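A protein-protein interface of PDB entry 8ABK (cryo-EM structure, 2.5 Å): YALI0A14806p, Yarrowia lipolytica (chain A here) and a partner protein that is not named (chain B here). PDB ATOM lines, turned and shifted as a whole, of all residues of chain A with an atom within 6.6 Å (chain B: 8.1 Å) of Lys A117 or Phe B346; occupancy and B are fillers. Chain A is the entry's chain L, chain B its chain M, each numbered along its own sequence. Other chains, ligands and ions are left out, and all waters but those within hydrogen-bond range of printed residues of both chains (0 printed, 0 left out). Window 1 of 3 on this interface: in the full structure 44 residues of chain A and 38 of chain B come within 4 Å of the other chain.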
ATOM      1  N   THR A  51       1.363  22.634 -29.819  1.00  0.00           N
ATOM      2  CA  THR A  51       2.120  23.788 -30.260  1.00  0.00           C
ATOM      3  C   THR A  51       1.686  24.114 -31.686  1.00  0.00           C
ATOM      4  O   THR A  51       1.278  23.214 -32.410  1.00  0.00           O
ATOM      5  CB  THR A  51       3.607  23.451 -30.088  1.00  0.00           C
ATOM      6  OG1 THR A  51       4.006  24.072 -28.866  1.00  0.00           O
ATOM      7  CG2 THR A  51       4.481  23.809 -31.269  1.00  0.00           C
ATOM      8  N   ALA A  52       1.820  25.378 -32.109  1.00  0.00           N
ATOM      9  CA  ALA A  52       1.452  25.783 -33.458  1.00  0.00           C
ATOM     10  C   ALA A  52       2.568  26.597 -34.104  1.00  0.00           C
ATOM     11  O   ALA A  52       3.282  27.304 -33.417  1.00  0.00           O
ATOM     12  CB  ALA A  52       0.185  26.573 -33.388  1.00  0.00           C
ATOM     13  N   THR A  53       2.739  26.459 -35.421  1.00  0.00           N
ATOM     14  CA  THR A  53       3.605  27.346 -36.181  1.00  0.00           C
ATOM     15  C   THR A  53       2.738  28.185 -37.114  1.00  0.00           C
ATOM     16  O   THR A  53       2.195  27.648 -38.072  1.00  0.00           O
ATOM     17  CB  THR A  53       4.647  26.547 -36.976  1.00  0.00           C
ATOM     18  OG1 THR A  53       5.397  25.789 -36.025  1.00  0.00           O
ATOM     19  CG2 THR A  53       5.577  27.433 -37.773  1.00  0.00           C
ATOM     20  N   VAL A  54       2.598  29.485 -36.834  1.00  0.00           N
ATOM     21  CA  VAL A  54       1.979  30.398 -37.780  1.00  0.00           C
ATOM     22  C   VAL A  54       3.076  31.246 -38.390  1.00  0.00           C
ATOM     23  O   VAL A  54       4.022  31.628 -37.707  1.00  0.00           O
ATOM     24  CB  VAL A  54       0.908  31.300 -37.146  1.00  0.00           C
ATOM     25  CG1 VAL A  54      -0.248  30.479 -36.611  1.00  0.00           C
ATOM     26  CG2 VAL A  54       1.498  32.195 -36.071  1.00  0.00           C
ATOM     27  N   MET A  99       5.543  35.417 -24.669  1.00  0.00           N
ATOM     28  CA  MET A  99       4.754  34.438 -25.399  1.00  0.00           C
ATOM     29  C   MET A  99       5.152  33.041 -24.940  1.00  0.00           C
ATOM     30  O   MET A  99       4.293  32.205 -24.645  1.00  0.00           O
ATOM     31  CB  MET A  99       5.111  34.452 -26.882  1.00  0.00           C
ATOM     32  CG  MET A  99       4.205  35.172 -27.809  1.00  0.00           C
ATOM     33  SD  MET A  99       4.314  34.287 -29.419  1.00  0.00           S
ATOM     34  CE  MET A  99       6.046  33.800 -29.490  1.00  0.00           C
ATOM     35  N   GLY A 100       6.468  32.792 -24.919  1.00  0.00           N
ATOM     36  CA  GLY A 100       6.955  31.471 -24.577  1.00  0.00           C
ATOM     37  C   GLY A 100       7.650  30.764 -25.737  1.00  0.00           C
ATOM     38  O   GLY A 100       8.567  29.975 -25.508  1.00  0.00           O
ATOM     39  N   GLY A 101       7.208  31.039 -26.971  1.00  0.00           N
ATOM     40  CA  GLY A 101       7.802  30.417 -28.140  1.00  0.00           C
ATOM     41  C   GLY A 101       8.899  31.298 -28.725  1.00  0.00           C
ATOM     42  O   GLY A 101       9.493  32.097 -28.011  1.00  0.00           O
ATOM     43  N   HIS A 102       9.141  31.163 -30.028  1.00  0.00           N
ATOM     44  CA  HIS A 102      10.143  31.998 -30.669  1.00  0.00           C
ATOM     45  C   HIS A 102       9.639  32.470 -32.025  1.00  0.00           C
ATOM     46  O   HIS A 102       8.634  31.978 -32.525  1.00  0.00           O
ATOM     47  CB  HIS A 102      11.469  31.245 -30.806  1.00  0.00           C
ATOM     48  CG  HIS A 102      11.331  29.980 -31.579  1.00  0.00           C
ATOM     49  ND1 HIS A 102      10.954  28.794 -30.982  1.00  0.00           N
ATOM     50  CD2 HIS A 102      11.493  29.715 -32.891  1.00  0.00           C
ATOM     51  CE1 HIS A 102      10.900  27.847 -31.893  1.00  0.00           C
ATOM     52  NE2 HIS A 102      11.236  28.383 -33.074  1.00  0.00           N
ATOM     53  N   LEU A 103      10.359  33.436 -32.595  1.00  0.00           N
ATOM     54  CA  LEU A 103      10.131  33.893 -33.952  1.00  0.00           C
ATOM     55  C   LEU A 103      11.348  33.530 -34.785  1.00  0.00           C
ATOM     56  O   LEU A 103      12.448  33.411 -34.256  1.00  0.00           O
ATOM     57  CB  LEU A 103       9.958  35.407 -33.906  1.00  0.00           C
ATOM     58  CG  LEU A 103       8.524  35.920 -33.984  1.00  0.00           C
ATOM     59  CD1 LEU A 103       7.727  35.557 -32.738  1.00  0.00           C
ATOM     60  CD2 LEU A 103       8.559  37.431 -34.123  1.00  0.00           C
ATOM     61  N   ASN A 104      11.146  33.355 -36.089  1.00  0.00           N
ATOM     62  CA  ASN A 104      12.259  33.057 -36.964  1.00  0.00           C
ATOM     63  C   ASN A 104      11.981  33.618 -38.347  1.00  0.00           C
ATOM     64  O   ASN A 104      10.828  33.857 -38.684  1.00  0.00           O
ATOM     65  CB  ASN A 104      12.505  31.556 -37.024  1.00  0.00           C
ATOM     66  CG  ASN A 104      13.844  31.231 -37.640  1.00  0.00           C
ATOM     67  OD1 ASN A 104      14.814  31.969 -37.483  1.00  0.00           O
ATOM     68  ND2 ASN A 104      13.897  30.129 -38.367  1.00  0.00           N
ATOM     69  N   TYR A 115       8.116  33.397 -39.347  1.00  0.00           N
ATOM     70  CA  TYR A 115       7.141  32.575 -38.650  1.00  0.00           C
ATOM     71  C   TYR A 115       7.338  32.640 -37.148  1.00  0.00           C
ATOM     72  O   TYR A 115       8.365  33.104 -36.669  1.00  0.00           O
ATOM     73  CB  TYR A 115       7.124  31.138 -39.171  1.00  0.00           C
ATOM     74  CG  TYR A 115       8.369  30.349 -38.876  1.00  0.00           C
ATOM     75  CD1 TYR A 115       8.504  29.639 -37.691  1.00  0.00           C
ATOM     76  CD2 TYR A 115       9.402  30.291 -39.796  1.00  0.00           C
ATOM     77  CE1 TYR A 115       9.639  28.890 -37.425  1.00  0.00           C
ATOM     78  CE2 TYR A 115      10.556  29.568 -39.536  1.00  0.00           C
ATOM     79  CZ  TYR A 115      10.665  28.854 -38.354  1.00  0.00           C
ATOM     80  OH  TYR A 115      11.793  28.132 -38.098  1.00  0.00           O
ATOM     81  N   ALA A 116       6.351  32.103 -36.431  1.00  0.00           N
ATOM     82  CA  ALA A 116       6.325  32.157 -34.987  1.00  0.00           C
ATOM     83  C   ALA A 116       5.849  30.808 -34.486  1.00  0.00           C
ATOM     84  O   ALA A 116       4.758  30.374 -34.849  1.00  0.00           O
ATOM     85  CB  ALA A 116       5.375  33.236 -34.566  1.00  0.00           C
ATOM     86  N   LYS A 117       6.685  30.145 -33.691  1.00  0.00           N
ATOM     87  CA  LYS A 117       6.267  28.911 -33.060  1.00  0.00           C
ATOM     88  C   LYS A 117       5.814  29.249 -31.648  1.00  0.00           C
ATOM     89  O   LYS A 117       6.511  29.968 -30.943  1.00  0.00           O
ATOM     90  CB  LYS A 117       7.414  27.904 -33.087  1.00  0.00           C
ATOM     91  CG  LYS A 117       6.979  26.464 -32.912  1.00  0.00           C
ATOM     92  CD  LYS A 117       8.136  25.517 -33.135  1.00  0.00           C
ATOM     93  CE  LYS A 117       7.894  24.093 -32.681  1.00  0.00           C
ATOM     94  NZ  LYS A 117       7.136  23.305 -33.683  1.00  0.00           N
ATOM     95  N   SER A 118       4.637  28.762 -31.255  1.00  0.00           N
ATOM     96  CA  SER A 118       4.116  29.114 -29.946  1.00  0.00           C
ATOM     97  C   SER A 118       3.327  27.954 -29.360  1.00  0.00           C
ATOM     98  O   SER A 118       3.376  26.835 -29.863  1.00  0.00           O
ATOM     99  CB  SER A 118       3.271  30.350 -30.026  1.00  0.00           C
ATOM    100  OG  SER A 118       2.178  30.126 -30.893  1.00  0.00           O
ATOM    101  N   PHE A 119       2.633  28.259 -28.261  1.00  0.00           N
ATOM    102  CA  PHE A 119       1.655  27.378 -27.661  1.00  0.00           C
ATOM    103  C   PHE A 119       0.327  27.573 -28.378  1.00  0.00           C
ATOM    104  O   PHE A 119       0.173  28.546 -29.106  1.00  0.00           O
ATOM    105  CB  PHE A 119       1.585  27.619 -26.151  1.00  0.00           C
ATOM    106  CG  PHE A 119       1.338  26.327 -25.426  1.00  0.00           C
ATOM    107  CD1 PHE A 119       2.355  25.390 -25.315  1.00  0.00           C
ATOM    108  CD2 PHE A 119       0.069  25.993 -24.974  1.00  0.00           C
ATOM    109  CE1 PHE A 119       2.114  24.161 -24.723  1.00  0.00           C
ATOM    110  CE2 PHE A 119      -0.168  24.762 -24.376  1.00  0.00           C
ATOM    111  CZ  PHE A 119       0.857  23.851 -24.254  1.00  0.00           C
ATOM    112  N   SER A 126       1.079  35.913 -31.486  1.00  0.00           N
ATOM    113  CA  SER A 126       2.122  35.723 -32.472  1.00  0.00           C
ATOM    114  C   SER A 126       1.701  36.277 -33.832  1.00  0.00           C
ATOM    115  O   SER A 126       2.511  36.917 -34.503  1.00  0.00           O
ATOM    116  CB  SER A 126       2.553  34.284 -32.507  1.00  0.00           C
ATOM    117  OG  SER A 126       1.431  33.423 -32.539  1.00  0.00           O
ATOM    118  N   GLY A 399       7.397  17.683 -37.828  1.00  0.00           N
ATOM    119  CA  GLY A 399       6.837  18.622 -36.872  1.00  0.00           C
ATOM    120  C   GLY A 399       6.067  19.738 -37.572  1.00  0.00           C
ATOM    121  O   GLY A 399       6.004  19.789 -38.800  1.00  0.00           O
ATOM    122  N   THR A 400       5.493  20.630 -36.762  1.00  0.00           N
ATOM    123  CA  THR A 400       4.607  21.669 -37.257  1.00  0.00           C
ATOM    124  C   THR A 400       5.365  22.628 -38.171  1.00  0.00           C
ATOM    125  O   THR A 400       4.775  23.176 -39.095  1.00  0.00           O
ATOM    126  CB  THR A 400       3.912  22.416 -36.113  1.00  0.00           C
ATOM    127  OG1 THR A 400       4.918  23.150 -35.422  1.00  0.00           O
ATOM    128  CG2 THR A 400       3.188  21.516 -35.136  1.00  0.00           C
ATOM    129  N   THR A 401       6.660  22.829 -37.906  1.00  0.00           N
ATOM    130  CA  THR A 401       7.432  23.783 -38.680  1.00  0.00           C
ATOM    131  C   THR A 401       7.662  23.240 -40.086  1.00  0.00           C
ATOM    132  O   THR A 401       7.626  24.006 -41.040  1.00  0.00           O
ATOM    133  CB  THR A 401       8.711  24.233 -37.963  1.00  0.00           C
ATOM    134  OG1 THR A 401       8.309  24.794 -36.718  1.00  0.00           O
ATOM    135  CG2 THR A 401       9.466  25.305 -38.719  1.00  0.00           C
ATOM    136  N   SER B 261      14.697  27.913 -17.848  1.00  0.00           N
ATOM    137  CA  SER B 261      14.042  28.621 -18.934  1.00  0.00           C
ATOM    138  C   SER B 261      14.023  30.120 -18.647  1.00  0.00           C
ATOM    139  O   SER B 261      14.288  30.907 -19.553  1.00  0.00           O
ATOM    140  CB  SER B 261      12.686  28.047 -19.238  1.00  0.00           C
ATOM    141  OG  SER B 261      12.058  27.589 -18.053  1.00  0.00           O
ATOM    142  N   SER B 268      15.119  34.547 -28.715  1.00  0.00           N
ATOM    143  CA  SER B 268      13.834  34.026 -29.135  1.00  0.00           C
ATOM    144  C   SER B 268      13.412  34.670 -30.452  1.00  0.00           C
ATOM    145  O   SER B 268      12.282  34.466 -30.896  1.00  0.00           O
ATOM    146  CB  SER B 268      12.816  34.192 -28.045  1.00  0.00           C
ATOM    147  OG  SER B 268      12.783  35.533 -27.579  1.00  0.00           O
ATOM    148  N   ARG B 339       6.808  34.752 -17.357  1.00  0.00           N
ATOM    149  CA  ARG B 339       7.664  34.502 -18.501  1.00  0.00           C
ATOM    150  C   ARG B 339       8.339  33.137 -18.349  1.00  0.00           C
ATOM    151  O   ARG B 339       8.550  32.456 -19.351  1.00  0.00           O
ATOM    152  CB  ARG B 339       8.625  35.679 -18.652  1.00  0.00           C
ATOM    153  CG  ARG B 339       9.718  35.504 -19.691  1.00  0.00           C
ATOM    154  CD  ARG B 339      10.260  36.843 -20.146  1.00  0.00           C
ATOM    155  NE  ARG B 339      10.150  38.005 -19.272  1.00  0.00           N
ATOM    156  CZ  ARG B 339      11.159  38.751 -18.835  1.00  0.00           C
ATOM    157  NH1 ARG B 339      12.405  38.480 -19.189  1.00  0.00           N
ATOM    158  NH2 ARG B 339      10.911  39.780 -18.045  1.00  0.00           N
ATOM    159  N   ALA B 340       8.611  32.714 -17.104  1.00  0.00           N
ATOM    160  CA  ALA B 340       9.302  31.449 -16.904  1.00  0.00           C
ATOM    161  C   ALA B 340       8.326  30.304 -17.121  1.00  0.00           C
ATOM    162  O   ALA B 340       8.697  29.266 -17.658  1.00  0.00           O
ATOM    163  CB  ALA B 340       9.933  31.366 -15.536  1.00  0.00           C
ATOM    164  N   TYR B 341       7.079  30.520 -16.708  1.00  0.00           N
ATOM    165  CA  TYR B 341       6.062  29.506 -16.875  1.00  0.00           C
ATOM    166  C   TYR B 341       5.793  29.301 -18.359  1.00  0.00           C
ATOM    167  O   TYR B 341       5.600  28.175 -18.795  1.00  0.00           O
ATOM    168  CB  TYR B 341       4.774  29.979 -16.217  1.00  0.00           C
ATOM    169  CG  TYR B 341       3.575  29.128 -16.525  1.00  0.00           C
ATOM    170  CD1 TYR B 341       3.549  27.793 -16.158  1.00  0.00           C
ATOM    171  CD2 TYR B 341       2.445  29.666 -17.124  1.00  0.00           C
ATOM    172  CE1 TYR B 341       2.437  27.002 -16.401  1.00  0.00           C
ATOM    173  CE2 TYR B 341       1.325  28.888 -17.375  1.00  0.00           C
ATOM    174  CZ  TYR B 341       1.320  27.551 -17.009  1.00  0.00           C
ATOM    175  OH  TYR B 341       0.226  26.767 -17.242  1.00  0.00           O
ATOM    176  N   ALA B 342       5.762  30.413 -19.099  1.00  0.00           N
ATOM    177  CA  ALA B 342       5.486  30.394 -20.523  1.00  0.00           C
ATOM    178  C   ALA B 342       6.597  29.656 -21.259  1.00  0.00           C
ATOM    179  O   ALA B 342       6.310  28.754 -22.032  1.00  0.00           O
ATOM    180  CB  ALA B 342       5.336  31.793 -21.057  1.00  0.00           C
ATOM    181  N   LYS B 343       7.850  30.065 -21.018  1.00  0.00           N
ATOM    182  CA  LYS B 343       9.000  29.474 -21.686  1.00  0.00           C
ATOM    183  C   LYS B 343       9.121  27.999 -21.317  1.00  0.00           C
ATOM    184  O   LYS B 343       9.538  27.195 -22.146  1.00  0.00           O
ATOM    185  CB  LYS B 343      10.297  30.228 -21.375  1.00  0.00           C
ATOM    186  CG  LYS B 343      10.367  31.635 -21.942  1.00  0.00           C
ATOM    187  CD  LYS B 343      11.662  31.913 -22.652  1.00  0.00           C
ATOM    188  CE  LYS B 343      12.626  32.738 -21.834  1.00  0.00           C
ATOM    189  NZ  LYS B 343      14.001  32.619 -22.373  1.00  0.00           N
ATOM    190  N   SER B 344       8.706  27.638 -20.098  1.00  0.00           N
ATOM    191  CA  SER B 344       8.872  26.264 -19.654  1.00  0.00           C
ATOM    192  C   SER B 344       7.776  25.354 -20.203  1.00  0.00           C
ATOM    193  O   SER B 344       8.079  24.221 -20.556  1.00  0.00           O
ATOM    194  CB  SER B 344       9.004  26.159 -18.161  1.00  0.00           C
ATOM    195  OG  SER B 344       7.778  26.484 -17.522  1.00  0.00           O
ATOM    196  N   LYS B 345       6.515  25.819 -20.226  1.00  0.00           N
ATOM    197  CA  LYS B 345       5.423  25.055 -20.817  1.00  0.00           C
ATOM    198  C   LYS B 345       5.749  24.752 -22.277  1.00  0.00           C
ATOM    199  O   LYS B 345       5.508  23.649 -22.762  1.00  0.00           O
ATOM    200  CB  LYS B 345       4.142  25.889 -20.852  1.00  0.00           C
ATOM    201  CG  LYS B 345       2.958  25.297 -20.114  1.00  0.00           C
ATOM    202  CD  LYS B 345       1.625  25.502 -20.814  1.00  0.00           C
ATOM    203  CE  LYS B 345       1.013  26.859 -20.537  1.00  0.00           C
ATOM    204  NZ  LYS B 345      -0.467  26.799 -20.542  1.00  0.00           N
ATOM    205  N   PHE B 346       6.272  25.766 -22.972  1.00  0.00           N
ATOM    206  CA  PHE B 346       6.583  25.634 -24.378  1.00  0.00           C
ATOM    207  C   PHE B 346       7.703  24.619 -24.558  1.00  0.00           C
ATOM    208  O   PHE B 346       7.625  23.796 -25.456  1.00  0.00           O
ATOM    209  CB  PHE B 346       6.975  26.976 -24.991  1.00  0.00           C
ATOM    210  CG  PHE B 346       7.330  26.881 -26.452  1.00  0.00           C
ATOM    211  CD1 PHE B 346       6.343  26.682 -27.413  1.00  0.00           C
ATOM    212  CD2 PHE B 346       8.650  26.958 -26.868  1.00  0.00           C
ATOM    213  CE1 PHE B 346       6.670  26.580 -28.758  1.00  0.00           C
ATOM    214  CE2 PHE B 346       8.976  26.878 -28.215  1.00  0.00           C
ATOM    215  CZ  PHE B 346       7.988  26.674 -29.155  1.00  0.00           C
ATOM    216  N   ALA B 347       8.742  24.688 -23.721  1.00  0.00           N
ATOM    217  CA  ALA B 347       9.843  23.745 -23.854  1.00  0.00           C
ATOM    218  C   ALA B 347       9.328  22.319 -23.668  1.00  0.00           C
ATOM    219  O   ALA B 347       9.750  21.410 -24.372  1.00  0.00           O
ATOM    220  CB  ALA B 347      10.949  24.057 -22.878  1.00  0.00           C
ATOM    221  N   ALA B 348       8.414  22.135 -22.717  1.00  0.00           N
ATOM    222  CA  ALA B 348       7.893  20.811 -22.449  1.00  0.00           C
ATOM    223  C   ALA B 348       7.106  20.314 -23.655  1.00  0.00           C
ATOM    224  O   ALA B 348       7.175  19.130 -23.964  1.00  0.00           O
ATOM    225  CB  ALA B 348       7.047  20.835 -21.211  1.00  0.00           C
ATOM    226  N   ALA B 349       6.368  21.221 -24.314  1.00  0.00           N
ATOM    227  CA  ALA B 349       5.476  20.843 -25.403  1.00  0.00           C
ATOM    228  C   ALA B 349       6.303  20.361 -26.586  1.00  0.00           C
ATOM    229  O   ALA B 349       6.077  19.267 -27.080  1.00  0.00           O
ATOM    230  CB  ALA B 349       4.550  21.974 -25.782  1.00  0.00           C
ATOM    231  N   GLU B 350       7.320  21.137 -26.953  1.00  0.00           N
ATOM    232  CA  GLU B 350       8.149  20.813 -28.102  1.00  0.00           C
ATOM    233  C   GLU B 350       9.002  19.566 -27.844  1.00  0.00           C
ATOM    234  O   GLU B 350       9.361  18.866 -28.791  1.00  0.00           O
ATOM    235  CB  GLU B 350       8.938  22.041 -28.550  1.00  0.00           C
ATOM    236  CG  GLU B 350      10.019  22.448 -27.570  1.00  0.00           C
ATOM    237  CD  GLU B 350      10.682  23.788 -27.818  1.00  0.00           C
ATOM    238  OE1 GLU B 350      11.105  24.422 -26.831  1.00  0.00           O
ATOM    239  OE2 GLU B 350      10.806  24.175 -28.995  1.00  0.00           O
ATOM    240  N   ALA B 351       9.307  19.268 -26.571  1.00  0.00           N
ATOM    241  CA  ALA B 351      10.038  18.055 -26.235  1.00  0.00           C
ATOM    242  C   ALA B 351       9.158  16.821 -26.421  1.00  0.00           C
ATOM    243  O   ALA B 351       9.634  15.780 -26.864  1.00  0.00           O
ATOM    244  CB  ALA B 351      10.612  18.130 -24.843  1.00  0.00           C
ATOM    245  N   PHE B 352       7.872  16.944 -26.091  1.00  0.00           N
ATOM    246  CA  PHE B 352       6.945  15.840 -26.267  1.00  0.00           C
ATOM    247  C   PHE B 352       6.587  15.669 -27.744  1.00  0.00           C
ATOM    248  O   PHE B 352       6.036  14.639 -28.124  1.00  0.00           O
ATOM    249  CB  PHE B 352       5.724  16.058 -25.375  1.00  0.00           C
ATOM    250  CG  PHE B 352       4.828  14.862 -25.209  1.00  0.00           C
ATOM    251  CD1 PHE B 352       5.340  13.660 -24.745  1.00  0.00           C
ATOM    252  CD2 PHE B 352       3.472  14.940 -25.505  1.00  0.00           C
ATOM    253  CE1 PHE B 352       4.513  12.557 -24.581  1.00  0.00           C
ATOM    254  CE2 PHE B 352       2.649  13.834 -25.352  1.00  0.00           C
ATOM    255  CZ  PHE B 352       3.171  12.642 -24.894  1.00  0.00           C
ATOM    256  N   GLU B 353       6.911  16.671 -28.572  1.00  0.00           N
ATOM    257  CA  GLU B 353       6.599  16.608 -29.992  1.00  0.00           C
ATOM    258  C   GLU B 353       7.747  15.959 -30.763  1.00  0.00           C
ATOM    259  O   GLU B 353       7.505  15.027 -31.531  1.00  0.00           O
ATOM    260  CB  GLU B 353       6.234  17.985 -30.544  1.00  0.00           C
ATOM    261  CG  GLU B 353       4.807  18.403 -30.227  1.00  0.00           C
ATOM    262  CD  GLU B 353       4.654  19.856 -29.789  1.00  0.00           C
ATOM    263  OE1 GLU B 353       5.457  20.695 -30.242  1.00  0.00           O
ATOM    264  OE2 GLU B 353       3.768  20.144 -28.943  1.00  0.00           O
ATOM    265  N   ASN B 354       8.981  16.441 -30.538  1.00  0.00           N
ATOM    266  CA  ASN B 354      10.172  15.915 -31.192  1.00  0.00           C
ATOM    267  C   ASN B 354      10.267  14.413 -30.931  1.00  0.00           C
ATOM    268  O   ASN B 354      10.346  14.006 -29.773  1.00  0.00           O
ATOM    269  CB  ASN B 354      11.448  16.639 -30.745  1.00  0.00           C
ATOM    270  CG  ASN B 354      12.730  15.949 -31.183  1.00  0.00           C
ATOM    271  OD1 ASN B 354      12.932  15.608 -32.346  1.00  0.00           O
ATOM    272  ND2 ASN B 354      13.613  15.722 -30.241  1.00  0.00           N
ATOM    273  N   PRO B 375       2.668  18.679 -20.975  1.00  0.00           N
ATOM    274  CA  PRO B 375       2.905  20.120 -21.102  1.00  0.00           C
ATOM    275  C   PRO B 375       1.791  21.006 -20.553  1.00  0.00           C
ATOM    276  O   PRO B 375       2.070  22.093 -20.053  1.00  0.00           O
ATOM    277  CB  PRO B 375       3.101  20.353 -22.609  1.00  0.00           C
ATOM    278  CG  PRO B 375       2.674  19.056 -23.260  1.00  0.00           C
ATOM    279  CD  PRO B 375       2.937  17.973 -22.235  1.00  0.00           C
ATOM    280  N   VAL B 378       2.263  21.436 -16.594  1.00  0.00           N
ATOM    281  CA  VAL B 378       3.505  22.011 -16.117  1.00  0.00           C
ATOM    282  C   VAL B 378       3.162  23.073 -15.080  1.00  0.00           C
ATOM    283  O   VAL B 378       2.328  23.937 -15.331  1.00  0.00           O
ATOM    284  CB  VAL B 378       4.309  22.564 -17.306  1.00  0.00           C
ATOM    285  CG1 VAL B 378       5.347  23.605 -16.915  1.00  0.00           C
ATOM    286  CG2 VAL B 378       4.941  21.429 -18.087  1.00  0.00           C
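Hydrophobic or aromatic side chains of chain A that line the printed part of chain B: His A102, Leu A103 and Phe A119.
Of the 20 printed residues of chain B, 7 touch a printed residue of chain A.
Hydrophobic or aromatic side chains of chain B within 4 Å of the printed part of chain A: Ala B342, Phe B346 and Ala B349.
Among the printed residues, no Asp or Glu carboxylate lies within 4 Å of a Lys or Arg side-chain nitrogen of the other chain.
The backbone NH (N) of Leu A103 lies within hydrogen-bond range of the backbone carbonyl oxygen (O) of Ser B268 (2.8 Å).
Among the printed residues, merely in contact across the chains: His A102 with Ser B268 (3.3 Å), Gly A100 with Phe B346 (3.3 Å), Thr A51 with Glu B353 (3.3 Å), Phe A119 with Ala B349 (3.4 Å), Ser A118 with Phe B346 (3.5 Å), Thr A51 with Phe B346 (3.7 Å), Gly A101 with Phe B346 (3.7 Å), Met A99 with Ala B342 (3.8 Å), Thr A51 with Ala B349 (3.8 Å), Gly A100 with Ala B342 (3.8 Å), Gly A100 with Lys B343 (3.9 Å), Phe A119 with Lys B345 (3.9 Å), Lys A117 with Phe B346 (3.9 Å), His A102 with Phe B346 (3.9 Å) and Gly A101 with Ser B268 (3.9 Å).
The backbone carbonyl oxygen (O) of Ser B261 sits at hydrogen-bond distance from the side-chain amino group (NZ) of Lys B343, at 3.3 Å.
The backbone carbonyl oxygen (O) of His A102 is in hydrogen-bond range of the backbone NH (N) of Lys A117 (2.9 Å).
The side-chain hydroxyl (OG1) of Thr A51 sits at hydrogen-bond distance from the backbone carbonyl oxygen (O) of Ser A118 (3.0 Å).
NZ of Lys B345 sits at hydrogen-bond distance from OH of Tyr B341.
OG1 of Thr A400 is in hydrogen-bond range of NZ of Lys A117 (2.8 Å).
The backbone carbonyl oxygen (O) of Ala A52 lies within hydrogen-bond range of the backbone NH (N) of Ser A118, 2.9 Å away.
Printed residues of chain B within 4 Å of Leu A103: Ser B268 (2.8 Å).
No residue of chain B comes within 4 Å of Ala A116.
Ser A118 touches one residue of chain B.
Of the printed residues of chain A, Ser B268 touches Gly A101, His A102 and Leu A103.
Of the printed residues of chain A, Ala B342 touches Met A99 (3.8 Å) and Gly A100 (3.8 Å).
Phe B346 touches just these residues of chain A: Thr A51 (3.7 Å), Gly A100 (3.3 Å), Gly A101 (3.7 Å), His A102 (3.9 Å), Lys A117 (3.9 Å) and Ser A118 (3.5 Å).
Of the printed residues of chain A, Glu B353 touches Thr A51 (3.3 Å).
The nearest residue of chain B that does not touch Lys A117 is Glu B353 (4.6 Å).
The nearest residue of chain A that does not touch Phe B346 is Phe A119 (4.1 Å).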
